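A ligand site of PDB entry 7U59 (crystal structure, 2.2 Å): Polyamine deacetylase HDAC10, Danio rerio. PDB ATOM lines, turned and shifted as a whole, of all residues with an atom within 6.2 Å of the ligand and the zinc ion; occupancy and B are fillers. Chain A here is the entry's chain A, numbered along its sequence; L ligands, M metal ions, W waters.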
ATOM      1  N   GLU A  24      24.074   9.368  18.524  1.00  0.00           N
ATOM      2  CA  GLU A  24      24.861  10.551  18.884  1.00  0.00           C
ATOM      3  C   GLU A  24      24.006  11.603  19.604  1.00  0.00           C
ATOM      4  O   GLU A  24      24.459  12.215  20.579  1.00  0.00           O
ATOM      5  CB  GLU A  24      25.507  11.138  17.629  1.00  0.00           C
ATOM      6  CG  GLU A  24      26.283  12.394  17.905  1.00  0.00           C
ATOM      7  CD  GLU A  24      26.921  12.974  16.659  1.00  0.00           C
ATOM      8  OE1 GLU A  24      26.357  12.817  15.545  1.00  0.00           O
ATOM      9  OE2 GLU A  24      27.990  13.603  16.802  1.00  0.00           O
ATOM     10  N   ILE A  27      21.102  11.414  23.708  1.00  0.00           N
ATOM     11  CA  ILE A  27      21.323  11.802  25.108  1.00  0.00           C
ATOM     12  C   ILE A  27      20.685  13.139  25.453  1.00  0.00           C
ATOM     13  O   ILE A  27      20.601  13.489  26.638  1.00  0.00           O
ATOM     14  CB  ILE A  27      22.817  11.928  25.437  1.00  0.00           C
ATOM     15  CG1 ILE A  27      23.493  12.817  24.385  1.00  0.00           C
ATOM     16  CG2 ILE A  27      23.485  10.554  25.533  1.00  0.00           C
ATOM     17  CD1 ILE A  27      24.856  13.293  24.775  1.00  0.00           C
ATOM     18  N   ASN A  93      26.500  19.590  12.249  1.00  0.00           N
ATOM     19  CA  ASN A  93      27.232  18.587  13.015  1.00  0.00           C
ATOM     20  C   ASN A  93      26.582  18.388  14.378  1.00  0.00           C
ATOM     21  O   ASN A  93      26.501  19.331  15.170  1.00  0.00           O
ATOM     22  CB  ASN A  93      28.692  19.032  13.183  1.00  0.00           C
ATOM     23  CG  ASN A  93      29.590  17.863  13.486  1.00  0.00           C
ATOM     24  OD1 ASN A  93      29.445  17.200  14.518  1.00  0.00           O
ATOM     25  ND2 ASN A  93      30.520  17.582  12.580  1.00  0.00           N
ATOM     26  N   ALA A  94      26.144  17.151  14.650  1.00  0.00           N
ATOM     27  CA  ALA A  94      25.673  16.733  15.973  1.00  0.00           C
ATOM     28  C   ALA A  94      24.494  17.581  16.467  1.00  0.00           C
ATOM     29  O   ALA A  94      24.519  18.215  17.529  1.00  0.00           O
ATOM     30  CB  ALA A  94      26.827  16.758  16.991  1.00  0.00           C
ATOM     31  N   PRO A 134      20.536  23.998  24.426  1.00  0.00           N
ATOM     32  CA  PRO A 134      21.717  24.743  24.873  1.00  0.00           C
ATOM     33  C   PRO A 134      22.228  25.667  23.777  1.00  0.00           C
ATOM     34  O   PRO A 134      21.674  25.673  22.674  1.00  0.00           O
ATOM     35  CB  PRO A 134      22.735  23.635  25.202  1.00  0.00           C
ATOM     36  CG  PRO A 134      22.355  22.505  24.277  1.00  0.00           C
ATOM     37  CD  PRO A 134      20.835  22.579  24.139  1.00  0.00           C
ATOM     38  N   HIS A 136      26.101  27.044  23.472  1.00  0.00           N
ATOM     39  CA  HIS A 136      27.461  27.568  23.376  1.00  0.00           C
ATOM     40  C   HIS A 136      28.222  27.072  22.130  1.00  0.00           C
ATOM     41  O   HIS A 136      29.196  27.706  21.744  1.00  0.00           O
ATOM     42  CB  HIS A 136      28.263  27.299  24.670  1.00  0.00           C
ATOM     43  CG  HIS A 136      28.621  25.861  24.922  1.00  0.00           C
ATOM     44  ND1 HIS A 136      29.743  25.502  25.654  1.00  0.00           N
ATOM     45  CD2 HIS A 136      28.012  24.708  24.584  1.00  0.00           C
ATOM     46  CE1 HIS A 136      29.807  24.183  25.734  1.00  0.00           C
ATOM     47  NE2 HIS A 136      28.766  23.678  25.109  1.00  0.00           N
ATOM     48  N   HIS A 137      27.743  26.029  21.471  1.00  0.00           N
ATOM     49  CA  HIS A 137      28.306  25.615  20.189  1.00  0.00           C
ATOM     50  C   HIS A 137      27.736  26.350  18.972  1.00  0.00           C
ATOM     51  O   HIS A 137      28.353  26.307  17.907  1.00  0.00           O
ATOM     52  CB  HIS A 137      28.077  24.128  19.978  1.00  0.00           C
ATOM     53  CG  HIS A 137      28.765  23.274  20.989  1.00  0.00           C
ATOM     54  ND1 HIS A 137      30.109  23.416  21.271  1.00  0.00           N
ATOM     55  CD2 HIS A 137      28.305  22.290  21.795  1.00  0.00           C
ATOM     56  CE1 HIS A 137      30.445  22.565  22.216  1.00  0.00           C
ATOM     57  NE2 HIS A 137      29.374  21.860  22.542  1.00  0.00           N
ATOM     58  N   GLY A 145      26.154  20.819  17.734  1.00  0.00           N
ATOM     59  CA  GLY A 145      26.249  20.209  19.047  1.00  0.00           C
ATOM     60  C   GLY A 145      25.046  20.467  19.940  1.00  0.00           C
ATOM     61  O   GLY A 145      25.218  20.978  21.046  1.00  0.00           O
ATOM     62  N   PHE A 146      23.832  20.162  19.448  1.00  0.00           N
ATOM     63  CA  PHE A 146      22.561  20.344  20.146  1.00  0.00           C
ATOM     64  C   PHE A 146      22.123  21.804  20.235  1.00  0.00           C
ATOM     65  O   PHE A 146      21.012  22.068  20.708  1.00  0.00           O
ATOM     66  CB  PHE A 146      22.584  19.785  21.582  1.00  0.00           C
ATOM     67  CG  PHE A 146      22.959  18.346  21.668  1.00  0.00           C
ATOM     68  CD1 PHE A 146      22.818  17.514  20.570  1.00  0.00           C
ATOM     69  CD2 PHE A 146      23.456  17.808  22.848  1.00  0.00           C
ATOM     70  CE1 PHE A 146      23.164  16.184  20.642  1.00  0.00           C
ATOM     71  CE2 PHE A 146      23.761  16.481  22.940  1.00  0.00           C
ATOM     72  CZ  PHE A 146      23.625  15.666  21.816  1.00  0.00           C
ATOM     73  N   CYS A 147      22.965  22.745  19.804  1.00  0.00           N
ATOM     74  CA  CYS A 147      22.725  24.169  19.990  1.00  0.00           C
ATOM     75  C   CYS A 147      22.144  24.780  18.716  1.00  0.00           C
ATOM     76  O   CYS A 147      22.661  24.524  17.626  1.00  0.00           O
ATOM     77  CB  CYS A 147      24.023  24.891  20.346  1.00  0.00           C
ATOM     78  SG  CYS A 147      24.769  24.302  21.863  1.00  0.00           S
ATOM     79  N   ASP A 174      31.021  23.889  31.169  1.00  0.00           N
ATOM     80  CA  ASP A 174      30.648  22.711  30.402  1.00  0.00           C
ATOM     81  C   ASP A 174      31.916  21.967  30.010  1.00  0.00           C
ATOM     82  O   ASP A 174      32.983  22.581  29.865  1.00  0.00           O
ATOM     83  CB  ASP A 174      29.842  23.119  29.153  1.00  0.00           C
ATOM     84  CG  ASP A 174      29.208  21.946  28.411  1.00  0.00           C
ATOM     85  OD1 ASP A 174      27.987  21.730  28.567  1.00  0.00           O
ATOM     86  OD2 ASP A 174      29.885  21.258  27.617  1.00  0.00           O
ATOM     87  N   VAL A 175      31.812  20.641  29.858  1.00  0.00           N
ATOM     88  CA  VAL A 175      32.993  19.840  29.543  1.00  0.00           C
ATOM     89  C   VAL A 175      33.412  19.968  28.085  1.00  0.00           C
ATOM     90  O   VAL A 175      34.487  19.493  27.707  1.00  0.00           O
ATOM     91  CB  VAL A 175      32.743  18.367  29.903  1.00  0.00           C
ATOM     92  CG1 VAL A 175      32.018  17.630  28.750  1.00  0.00           C
ATOM     93  CG2 VAL A 175      34.046  17.673  30.258  1.00  0.00           C
ATOM     94  N   HIS A 176      32.571  20.547  27.245  1.00  0.00           N
ATOM     95  CA  HIS A 176      32.864  20.768  25.840  1.00  0.00           C
ATOM     96  C   HIS A 176      33.301  22.214  25.618  1.00  0.00           C
ATOM     97  O   HIS A 176      32.920  23.112  26.365  1.00  0.00           O
ATOM     98  CB  HIS A 176      31.642  20.460  24.962  1.00  0.00           C
ATOM     99  CG  HIS A 176      31.251  19.018  24.944  1.00  0.00           C
ATOM    100  ND1 HIS A 176      30.318  18.467  25.815  1.00  0.00           N
ATOM    101  CD2 HIS A 176      31.663  17.994  24.142  1.00  0.00           C
ATOM    102  CE1 HIS A 176      30.169  17.182  25.542  1.00  0.00           C
ATOM    103  NE2 HIS A 176      30.970  16.871  24.536  1.00  0.00           N
ATOM    104  N   HIS A 177      34.089  22.427  24.577  1.00  0.00           N
ATOM    105  CA  HIS A 177      34.551  23.767  24.244  1.00  0.00           C
ATOM    106  C   HIS A 177      33.428  24.574  23.584  1.00  0.00           C
ATOM    107  O   HIS A 177      32.859  24.128  22.585  1.00  0.00           O
ATOM    108  CB  HIS A 177      35.742  23.710  23.293  1.00  0.00           C
ATOM    109  CG  HIS A 177      36.260  25.065  22.900  1.00  0.00           C
ATOM    110  ND1 HIS A 177      36.600  25.396  21.608  1.00  0.00           N
ATOM    111  CD2 HIS A 177      36.510  26.162  23.653  1.00  0.00           C
ATOM    112  CE1 HIS A 177      37.018  26.650  21.571  1.00  0.00           C
ATOM    113  NE2 HIS A 177      36.994  27.133  22.800  1.00  0.00           N
ATOM    114  N   TRP A 205      35.566  15.675  20.426  1.00  0.00           N
ATOM    115  CA  TRP A 205      34.669  16.606  19.752  1.00  0.00           C
ATOM    116  C   TRP A 205      34.677  17.953  20.470  1.00  0.00           C
ATOM    117  O   TRP A 205      34.654  17.995  21.712  1.00  0.00           O
ATOM    118  CB  TRP A 205      33.253  16.004  19.719  1.00  0.00           C
ATOM    119  CG  TRP A 205      32.341  16.690  18.755  1.00  0.00           C
ATOM    120  CD1 TRP A 205      32.104  16.331  17.456  1.00  0.00           C
ATOM    121  CD2 TRP A 205      31.558  17.858  19.004  1.00  0.00           C
ATOM    122  NE1 TRP A 205      31.221  17.216  16.882  1.00  0.00           N
ATOM    123  CE2 TRP A 205      30.882  18.170  17.806  1.00  0.00           C
ATOM    124  CE3 TRP A 205      31.378  18.694  20.124  1.00  0.00           C
ATOM    125  CZ2 TRP A 205      30.026  19.270  17.690  1.00  0.00           C
ATOM    126  CZ3 TRP A 205      30.530  19.802  19.999  1.00  0.00           C
ATOM    127  CH2 TRP A 205      29.863  20.075  18.790  1.00  0.00           C
ATOM    128  N   GLY A 265      27.408  23.906  31.907  1.00  0.00           N
ATOM    129  CA  GLY A 265      27.122  22.539  31.518  1.00  0.00           C
ATOM    130  C   GLY A 265      27.629  21.640  32.627  1.00  0.00           C
ATOM    131  O   GLY A 265      28.726  21.838  33.148  1.00  0.00           O
ATOM    132  N   ASP A 267      27.879  18.366  32.271  1.00  0.00           N
ATOM    133  CA  ASP A 267      28.554  17.191  31.757  1.00  0.00           C
ATOM    134  C   ASP A 267      30.019  17.155  32.160  1.00  0.00           C
ATOM    135  O   ASP A 267      30.698  16.180  31.830  1.00  0.00           O
ATOM    136  CB  ASP A 267      28.406  17.068  30.228  1.00  0.00           C
ATOM    137  CG  ASP A 267      28.741  18.341  29.469  1.00  0.00           C
ATOM    138  OD1 ASP A 267      29.301  19.300  30.043  1.00  0.00           O
ATOM    139  OD2 ASP A 267      28.448  18.364  28.249  1.00  0.00           O
ATOM    140  N   GLU A 274      29.336  11.803  28.466  1.00  0.00           N
ATOM    141  CA  GLU A 274      30.110  12.514  27.470  1.00  0.00           C
ATOM    142  C   GLU A 274      31.423  13.042  28.027  1.00  0.00           C
ATOM    143  O   GLU A 274      32.459  12.969  27.351  1.00  0.00           O
ATOM    144  CB  GLU A 274      29.301  13.672  26.889  1.00  0.00           C
ATOM    145  CG  GLU A 274      28.134  13.237  26.045  1.00  0.00           C
ATOM    146  CD  GLU A 274      28.555  12.307  24.899  1.00  0.00           C
ATOM    147  OE1 GLU A 274      29.514  12.645  24.170  1.00  0.00           O
ATOM    148  OE2 GLU A 274      27.907  11.242  24.734  1.00  0.00           O
ATOM    149  N   GLU A 304      23.790  24.697  29.976  1.00  0.00           N
ATOM    150  CA  GLU A 304      24.226  24.172  28.687  1.00  0.00           C
ATOM    151  C   GLU A 304      23.953  22.675  28.688  1.00  0.00           C
ATOM    152  O   GLU A 304      22.786  22.264  28.581  1.00  0.00           O
ATOM    153  CB  GLU A 304      25.682  24.553  28.434  1.00  0.00           C
ATOM    154  CG  GLU A 304      25.927  26.078  28.396  1.00  0.00           C
ATOM    155  CD  GLU A 304      25.625  26.682  27.011  1.00  0.00           C
ATOM    156  OE1 GLU A 304      25.221  25.928  26.108  1.00  0.00           O
ATOM    157  OE2 GLU A 304      25.853  27.896  26.808  1.00  0.00           O
ATOM    158  N   GLY A 305      24.982  21.824  28.801  1.00  0.00           N
ATOM    159  CA  GLY A 305      24.798  20.377  28.756  1.00  0.00           C
ATOM    160  C   GLY A 305      24.710  19.720  30.132  1.00  0.00           C
ATOM    161  O   GLY A 305      24.554  20.374  31.167  1.00  0.00           O
ATOM    162  N   GLY A 306      24.828  18.385  30.123  1.00  0.00           N
ATOM    163  CA  GLY A 306      24.736  17.572  31.340  1.00  0.00           C
ATOM    164  C   GLY A 306      23.729  16.455  31.137  1.00  0.00           C
ATOM    165  O   GLY A 306      22.539  16.728  30.963  1.00  0.00           O
ATOM    166  N   TYR A 307      24.170  15.192  31.138  1.00  0.00           N
ATOM    167  CA  TYR A 307      23.371  14.116  30.561  1.00  0.00           C
ATOM    168  C   TYR A 307      23.154  12.922  31.474  1.00  0.00           C
ATOM    169  O   TYR A 307      22.396  12.024  31.110  1.00  0.00           O
ATOM    170  CB  TYR A 307      24.017  13.619  29.252  1.00  0.00           C
ATOM    171  CG  TYR A 307      24.242  14.784  28.333  1.00  0.00           C
ATOM    172  CD1 TYR A 307      23.165  15.332  27.644  1.00  0.00           C
ATOM    173  CD2 TYR A 307      25.492  15.370  28.211  1.00  0.00           C
ATOM    174  CE1 TYR A 307      23.326  16.430  26.826  1.00  0.00           C
ATOM    175  CE2 TYR A 307      25.672  16.479  27.383  1.00  0.00           C
ATOM    176  CZ  TYR A 307      24.590  17.002  26.693  1.00  0.00           C
ATOM    177  OH  TYR A 307      24.735  18.088  25.870  1.00  0.00           O
HETATM  178  C1  LIG L   1      29.322  14.832  19.768  1.00  0.00           C
HETATM  179  C2  LIG L   1      30.855  11.926  17.791  1.00  0.00           C
HETATM  180  C3  LIG L   1      30.334  10.204  16.175  1.00  0.00           C
HETATM  181  C4  LIG L   1      31.951   9.777  17.891  1.00  0.00           C
HETATM  182  C5  LIG L   1      27.944  18.330  22.129  1.00  0.00           C
HETATM  183  C6  LIG L   1      27.443  18.995  24.467  1.00  0.00           C
HETATM  184  C7  LIG L   1      27.170  17.990  23.304  1.00  0.00           C
HETATM  185  C8  LIG L   1      27.377  16.631  23.757  1.00  0.00           C
HETATM  186  C9  LIG L   1      27.368  15.571  22.633  1.00  0.00           C
HETATM  187  C10 LIG L   1      28.031  15.060  20.577  1.00  0.00           C
HETATM  188  C11 LIG L   1      30.635  13.347  18.358  1.00  0.00           C
HETATM  189  C12 LIG L   1      30.149  11.482  16.676  1.00  0.00           C
HETATM  190  C13 LIG L   1      31.243   9.342  16.782  1.00  0.00           C
HETATM  191  C14 LIG L   1      31.756  11.053  18.393  1.00  0.00           C
HETATM  192  C15 LIG L   1      28.170  17.239  21.052  1.00  0.00           C
HETATM  193  N1  LIG L   1      27.943  20.315  24.221  1.00  0.00           N
HETATM  194  N2  LIG L   1      28.207  15.860  21.488  1.00  0.00           N
HETATM  195  N3  LIG L   1      29.502  13.453  19.291  1.00  0.00           N
HETATM  196  O1  LIG L   1      28.174  21.195  25.296  1.00  0.00           O
HETATM  197  O2  LIG L   1      27.264  18.713  25.608  1.00  0.00           O
HETATM  198 ZN    ZN M   1      28.800  19.837  26.902  1.00  0.00          ZN
HETATM  199  O   HOH W   1      30.500  14.696  23.187  1.00  0.00           O
HETATM  200  O   HOH W   2      28.931  11.177  20.470  1.00  0.00           O
HETATM  201  O   HOH W   3      32.039  12.977  21.334  1.00  0.00           O
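NE2 of His 136 lies close to O1 of the ligand, 2.6 Å away. OE2 of Glu 24 is in salt-bridge range of N3 of the ligand (2.9 Å). The side-chain hydroxyl (OH) of Tyr 307 lies close to an oxygen (O2) of the ligand. A nitrogen (N1) of the ligand is in hydrogen-bond range of a ring nitrogen (NE2) of His 137, at 2.7 Å.
The backbone carbonyl oxygen of Ala 94 sits at hydrogen-bond distance from the backbone NH of Phe 146 (2.8 Å). N of Gly 145 sits at hydrogen-bond distance from O of Asn 93. The backbone carbonyl oxygen (O) of Gly 145 lies within hydrogen-bond range of the side-chain sulfur (SG) of Cys 147, 3.5 Å away. The backbone NH (N) of Gly 145 lies close to the backbone carbonyl oxygen (O) of Ala 94, 3.1 Å away. The backbone carbonyl oxygen (O) of His 177 sits close to a ring nitrogen (ND1) of His 137, at 3.1 Å. The side-chain sulfur of Cys 147 sits at hydrogen-bond distance from the backbone NH of His 137, 3.5 Å away. The backbone NH of Val 175 is in hydrogen-bond range of the side-chain carboxylate of Asp 267, 2.9 Å away. The backbone NH (N) of Gly 305 is in hydrogen-bond range of the side-chain carboxylate (OD1) of Asp 174, at 3.0 Å.
Residues that only touch the ligand: Gly 145, Phe 146, Trp 205 and Glu 274. Of the 22 residues printed, 11 come within 4 Å of the ligand. The nearest printed residue that does not touch the ligand is Ile 27 (4.01 Å).
Of the 22 residues printed, 3 come within 4 Å of the zinc ion. Along chain A the residues within 4 Å of the zinc ion span positions 174 to 267. The nearest printed residue that does not touch the zinc ion is His 136 (4.2 Å).
The zinc ion is bound by the side-chain carboxylate of Asp 174 (1.9 Å), the side-chain carboxylate of Asp 267 (2.0 Å), an oxygen (O1) of the ligand (2.2 Å), an oxygen (O2) of the ligand (2.3 Å) and a ring nitrogen (ND1) of His 176 (2.3 Å). The zinc ion has five donor atoms within binding distance. Slightly farther from the zinc ion lies the side-chain carboxylate (OD1) of Asp 174 (2.6 Å).
Water W1 lies within hydrogen-bond range of the side-chain carboxylate (OE1) of Glu 274 (2.5 Å) and a ring nitrogen (NE2) of His 176 (2.6 Å).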
